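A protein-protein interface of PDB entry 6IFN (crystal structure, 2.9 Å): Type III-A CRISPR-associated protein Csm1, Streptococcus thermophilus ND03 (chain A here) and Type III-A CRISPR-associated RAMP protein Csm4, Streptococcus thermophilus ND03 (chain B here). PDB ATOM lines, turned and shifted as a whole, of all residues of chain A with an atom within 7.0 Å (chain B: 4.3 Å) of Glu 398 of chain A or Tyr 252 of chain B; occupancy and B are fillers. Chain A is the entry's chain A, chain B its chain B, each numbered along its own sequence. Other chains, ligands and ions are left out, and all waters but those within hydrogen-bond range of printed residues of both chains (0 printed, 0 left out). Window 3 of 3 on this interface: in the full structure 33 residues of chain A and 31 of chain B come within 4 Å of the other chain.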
ATOM      1  N   SER A 396     -20.138  12.514  16.184  1.00  0.00           N
ATOM      2  CA  SER A 396     -19.251  13.110  15.218  1.00  0.00           C
ATOM      3  C   SER A 396     -19.819  14.472  14.866  1.00  0.00           C
ATOM      4  O   SER A 396     -20.636  14.571  13.993  1.00  0.00           O
ATOM      5  CB  SER A 396     -19.098  12.277  13.976  1.00  0.00           C
ATOM      6  OG  SER A 396     -20.144  12.539  13.057  1.00  0.00           O
ATOM      7  N   SER A 397     -19.378  15.499  15.580  1.00  0.00           N
ATOM      8  CA  SER A 397     -20.033  16.787  15.534  1.00  0.00           C
ATOM      9  C   SER A 397     -19.097  17.815  14.907  1.00  0.00           C
ATOM     10  O   SER A 397     -17.998  18.019  15.343  1.00  0.00           O
ATOM     11  CB  SER A 397     -20.479  17.193  16.920  1.00  0.00           C
ATOM     12  OG  SER A 397     -21.479  18.202  16.862  1.00  0.00           O
ATOM     13  N   GLU A 398     -19.584  18.463  13.870  1.00  0.00           N
ATOM     14  CA  GLU A 398     -18.795  19.428  13.158  1.00  0.00           C
ATOM     15  C   GLU A 398     -18.774  20.752  13.912  1.00  0.00           C
ATOM     16  O   GLU A 398     -17.813  21.473  13.776  1.00  0.00           O
ATOM     17  CB  GLU A 398     -19.398  19.686  11.782  1.00  0.00           C
ATOM     18  CG  GLU A 398     -18.389  20.099  10.725  1.00  0.00           C
ATOM     19  CD  GLU A 398     -18.928  19.758   9.347  1.00  0.00           C
ATOM     20  OE1 GLU A 398     -19.096  18.522   9.061  1.00  0.00           O
ATOM     21  OE2 GLU A 398     -19.256  20.726   8.592  1.00  0.00           O
ATOM     22  N   ARG A 399     -19.844  21.041  14.663  1.00  0.00           N
ATOM     23  CA  ARG A 399     -20.028  22.339  15.270  1.00  0.00           C
ATOM     24  C   ARG A 399     -20.293  22.221  16.775  1.00  0.00           C
ATOM     25  O   ARG A 399     -20.549  21.158  17.298  1.00  0.00           O
ATOM     26  CB  ARG A 399     -21.161  23.045  14.539  1.00  0.00           C
ATOM     27  CG  ARG A 399     -20.907  23.105  13.043  1.00  0.00           C
ATOM     28  CD  ARG A 399     -21.599  24.260  12.384  1.00  0.00           C
ATOM     29  NE  ARG A 399     -21.196  25.490  13.046  1.00  0.00           N
ATOM     30  CZ  ARG A 399     -21.756  26.672  12.829  1.00  0.00           C
ATOM     31  NH1 ARG A 399     -22.734  26.779  11.942  1.00  0.00           N
ATOM     32  NH2 ARG A 399     -21.332  27.728  13.504  1.00  0.00           N
ATOM     33  N   GLU A 400     -20.224  23.355  17.468  1.00  0.00           N
ATOM     34  CA  GLU A 400     -20.419  23.420  18.920  1.00  0.00           C
ATOM     35  C   GLU A 400     -21.150  24.726  19.255  1.00  0.00           C
ATOM     36  O   GLU A 400     -21.255  25.589  18.402  1.00  0.00           O
ATOM     37  CB  GLU A 400     -19.057  23.360  19.599  1.00  0.00           C
ATOM     38  CG  GLU A 400     -18.242  24.624  19.406  1.00  0.00           C
ATOM     39  CD  GLU A 400     -16.749  24.418  19.523  1.00  0.00           C
ATOM     40  OE1 GLU A 400     -16.343  23.358  19.993  1.00  0.00           O
ATOM     41  OE2 GLU A 400     -16.000  25.314  19.144  1.00  0.00           O
ATOM     42  N   VAL A 407     -21.730  20.481  22.749  1.00  0.00           N
ATOM     43  CA  VAL A 407     -22.171  19.788  21.541  1.00  0.00           C
ATOM     44  C   VAL A 407     -23.517  19.102  21.801  1.00  0.00           C
ATOM     45  O   VAL A 407     -23.927  18.276  20.988  1.00  0.00           O
ATOM     46  CB  VAL A 407     -21.141  18.747  21.066  1.00  0.00           C
ATOM     47  CG1 VAL A 407     -19.895  19.386  20.482  1.00  0.00           C
ATOM     48  CG2 VAL A 407     -20.767  17.796  22.181  1.00  0.00           C
ATOM     49  N   PHE B 242     -10.892  19.781  18.605  1.00  0.00           N
ATOM     50  CA  PHE B 242     -11.088  19.429  17.227  1.00  0.00           C
ATOM     51  C   PHE B 242      -9.887  18.595  16.780  1.00  0.00           C
ATOM     52  O   PHE B 242      -8.781  18.924  17.043  1.00  0.00           O
ATOM     53  CB  PHE B 242     -11.250  20.710  16.410  1.00  0.00           C
ATOM     54  CG  PHE B 242     -12.612  21.345  16.521  1.00  0.00           C
ATOM     55  CD1 PHE B 242     -12.880  22.288  17.495  1.00  0.00           C
ATOM     56  CD2 PHE B 242     -13.628  21.015  15.635  1.00  0.00           C
ATOM     57  CE1 PHE B 242     -14.137  22.868  17.590  1.00  0.00           C
ATOM     58  CE2 PHE B 242     -14.881  21.602  15.728  1.00  0.00           C
ATOM     59  CZ  PHE B 242     -15.139  22.519  16.714  1.00  0.00           C
ATOM     60  N   ALA B 243     -10.124  17.479  16.115  1.00  0.00           N
ATOM     61  CA  ALA B 243      -9.056  16.579  15.765  1.00  0.00           C
ATOM     62  C   ALA B 243      -8.218  17.227  14.675  1.00  0.00           C
ATOM     63  O   ALA B 243      -8.725  17.594  13.654  1.00  0.00           O
ATOM     64  CB  ALA B 243      -9.632  15.273  15.295  1.00  0.00           C
ATOM     65  N   GLU B 250     -13.076  19.532   6.508  1.00  0.00           N
ATOM     66  CA  GLU B 250     -13.980  19.917   7.600  1.00  0.00           C
ATOM     67  C   GLU B 250     -13.297  19.622   8.944  1.00  0.00           C
ATOM     68  O   GLU B 250     -12.371  18.787   8.993  1.00  0.00           O
ATOM     69  CB  GLU B 250     -15.319  19.187   7.506  1.00  0.00           C
ATOM     70  CG  GLU B 250     -16.035  19.360   6.185  1.00  0.00           C
ATOM     71  CD  GLU B 250     -15.341  18.656   5.030  1.00  0.00           C
ATOM     72  OE1 GLU B 250     -15.112  17.414   5.129  1.00  0.00           O
ATOM     73  OE2 GLU B 250     -14.990  19.363   4.047  1.00  0.00           O
ATOM     74  N   ASN B 251     -13.764  20.271  10.025  1.00  0.00           N
ATOM     75  CA  ASN B 251     -13.243  20.013  11.401  1.00  0.00           C
ATOM     76  C   ASN B 251     -14.316  19.386  12.294  1.00  0.00           C
ATOM     77  O   ASN B 251     -15.450  19.904  12.449  1.00  0.00           O
ATOM     78  CB  ASN B 251     -12.714  21.289  12.024  1.00  0.00           C
ATOM     79  CG  ASN B 251     -11.499  21.735  11.258  1.00  0.00           C
ATOM     80  OD1 ASN B 251     -10.595  20.939  11.045  1.00  0.00           O
ATOM     81  ND2 ASN B 251     -11.491  22.971  10.809  1.00  0.00           N
ATOM     82  N   TYR B 252     -13.974  18.233  12.864  1.00  0.00           N
ATOM     83  CA  TYR B 252     -14.896  17.527  13.715  1.00  0.00           C
ATOM     84  C   TYR B 252     -14.326  17.519  15.127  1.00  0.00           C
ATOM     85  O   TYR B 252     -13.153  17.238  15.334  1.00  0.00           O
ATOM     86  CB  TYR B 252     -15.103  16.101  13.220  1.00  0.00           C
ATOM     87  CG  TYR B 252     -15.674  16.008  11.831  1.00  0.00           C
ATOM     88  CD1 TYR B 252     -14.899  16.272  10.722  1.00  0.00           C
ATOM     89  CD2 TYR B 252     -16.996  15.636  11.628  1.00  0.00           C
ATOM     90  CE1 TYR B 252     -15.436  16.177   9.447  1.00  0.00           C
ATOM     91  CE2 TYR B 252     -17.543  15.520  10.363  1.00  0.00           C
ATOM     92  CZ  TYR B 252     -16.768  15.812   9.256  1.00  0.00           C
ATOM     93  OH  TYR B 252     -17.322  15.711   7.997  1.00  0.00           O
ATOM     94  N   ARG B 253     -15.182  17.822  16.095  1.00  0.00           N
ATOM     95  CA  ARG B 253     -14.859  17.648  17.471  1.00  0.00           C
ATOM     96  C   ARG B 253     -14.543  16.178  17.684  1.00  0.00           C
ATOM     97  O   ARG B 253     -15.333  15.349  17.319  1.00  0.00           O
ATOM     98  CB  ARG B 253     -16.038  18.090  18.342  1.00  0.00           C
ATOM     99  CG  ARG B 253     -16.009  19.581  18.671  1.00  0.00           C
ATOM    100  CD  ARG B 253     -15.103  19.922  19.848  1.00  0.00           C
ATOM    101  NE  ARG B 253     -15.713  19.525  21.116  1.00  0.00           N
ATOM    102  CZ  ARG B 253     -16.694  20.204  21.715  1.00  0.00           C
ATOM    103  NH1 ARG B 253     -17.159  21.316  21.181  1.00  0.00           N
ATOM    104  NH2 ARG B 253     -17.195  19.789  22.861  1.00  0.00           N
ATOM    105  N   LYS B 254     -13.379  15.877  18.249  1.00  0.00           N
ATOM    106  CA  LYS B 254     -13.178  14.543  18.780  1.00  0.00           C
ATOM    107  C   LYS B 254     -14.097  14.325  19.995  1.00  0.00           C
ATOM    108  O   LYS B 254     -14.764  15.258  20.485  1.00  0.00           O
ATOM    109  CB  LYS B 254     -11.715  14.250  19.109  1.00  0.00           C
ATOM    110  CG  LYS B 254     -10.868  15.418  19.511  1.00  0.00           C
ATOM    111  CD  LYS B 254      -9.415  15.063  19.428  1.00  0.00           C
ATOM    112  CE  LYS B 254      -8.575  15.744  20.495  1.00  0.00           C
ATOM    113  NZ  LYS B 254      -7.145  15.801  20.098  1.00  0.00           N
ATOM    114  N   PRO B 279     -13.934  11.176  15.722  1.00  0.00           N
ATOM    115  CA  PRO B 279     -15.335  11.345  15.395  1.00  0.00           C
ATOM    116  C   PRO B 279     -15.791  10.020  14.801  1.00  0.00           C
ATOM    117  O   PRO B 279     -15.027   9.468  14.053  1.00  0.00           O
ATOM    118  CB  PRO B 279     -15.329  12.440  14.319  1.00  0.00           C
ATOM    119  CG  PRO B 279     -14.023  13.167  14.530  1.00  0.00           C
ATOM    120  CD  PRO B 279     -13.061  12.103  14.996  1.00  0.00           C
ATOM    121  N   PHE B 282     -14.573   8.210  11.157  1.00  0.00           N
ATOM    122  CA  PHE B 282     -13.516   9.065  10.648  1.00  0.00           C
ATOM    123  C   PHE B 282     -12.455   8.212   9.964  1.00  0.00           C
ATOM    124  O   PHE B 282     -12.107   7.144  10.465  1.00  0.00           O
ATOM    125  CB  PHE B 282     -12.887   9.858  11.806  1.00  0.00           C
ATOM    126  CG  PHE B 282     -12.213  11.171  11.475  1.00  0.00           C
ATOM    127  CD1 PHE B 282     -12.960  12.303  11.188  1.00  0.00           C
ATOM    128  CD2 PHE B 282     -10.838  11.293  11.563  1.00  0.00           C
ATOM    129  CE1 PHE B 282     -12.339  13.506  10.911  1.00  0.00           C
ATOM    130  CE2 PHE B 282     -10.216  12.505  11.312  1.00  0.00           C
ATOM    131  CZ  PHE B 282     -10.967  13.606  10.978  1.00  0.00           C
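Of the printed residues of chain B, Glu 398 of chain A touches Phe 242 (3.5 Å), Asn 251 (3.1 Å) and Tyr 252 (3.5 Å). Tyr 252 of chain B touches just these residues of chain A: Ser 397 and Glu 398. Printed residues of chain A within 4 Å of Phe 242 of chain B: Glu 398 (3.5 Å) and Glu 400 (3.3 Å). Printed residues of chain B within 4 Å of Ser 396 of chain A: Pro 279 (3.8 Å). Printed residues of chain A within 4 Å of Pro 279 of chain B: Ser 396. Ala 243 of chain B touches none of the printed residues of chain A. The nearest printed residue of chain B that does not touch Ser 396 of chain A is Tyr 252 of chain B (4.5 Å).
The side-chain carboxylate of Glu 400 of chain A is in salt-bridge range of the guanidinium group of Arg 253 of chain B, at 2.5 Å. OE1 of Glu 398 of chain A is in hydrogen-bond range of OH of Tyr 252 of chain B, 3.5 Å away. The backbone carbonyl oxygen (O) of Glu 398 of chain A sits close to the backbone carbonyl oxygen (O) of Asn 251 of chain B, at 3.1 Å. The backbone carbonyl oxygen of Ser 397 of chain A is in hydrogen-bond range of the backbone NH of Arg 253 of chain B.
The backbone carbonyl oxygen (O) of Arg 399 of chain A is in hydrogen-bond range of the side-chain hydroxyl (OG) of Ser 397 of chain A. O of Tyr 252 of chain B sits at hydrogen-bond distance from N of Ala 243 of chain B, at 3.1 Å.
CB of Ser 396 of chain A touches CB of Pro 279 of chain B, 3.8 Å away. Ser 397 of chain A touches Tyr 252 of chain B (O to CA, 3.5 Å). O of Glu 398 of chain A touches CE2 of Phe 242 of chain B, at 3.5 Å. OE1 of Glu 400 of chain A touches CE1 of Phe 242 of chain B, at 3.3 Å. Arg 253 of chain B touches Val 407 of chain A (NH1 to CG1, 3.4 Å).
Printed residues of chain A that touch a printed residue of chain B: Ser 396, Ser 397, Glu 398, Glu 400 and Val 407. Hydrophobic or aromatic side chains of chain A within 4 Å of the printed part of chain B: Val 407. Of the 9 printed residues of chain B, 5 touch a printed residue of chain A. Hydrophobic or aromatic side chains of chain B within 4 Å of the printed part of chain A: Phe 242, Tyr 252 and Pro 279. Among the printed residues, Asp or Glu carboxylates within 4 Å of a Lys or Arg side-chain nitrogen of the other chain: Glu 400 of chain A with Arg 253 of chain B (2.5 Å).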
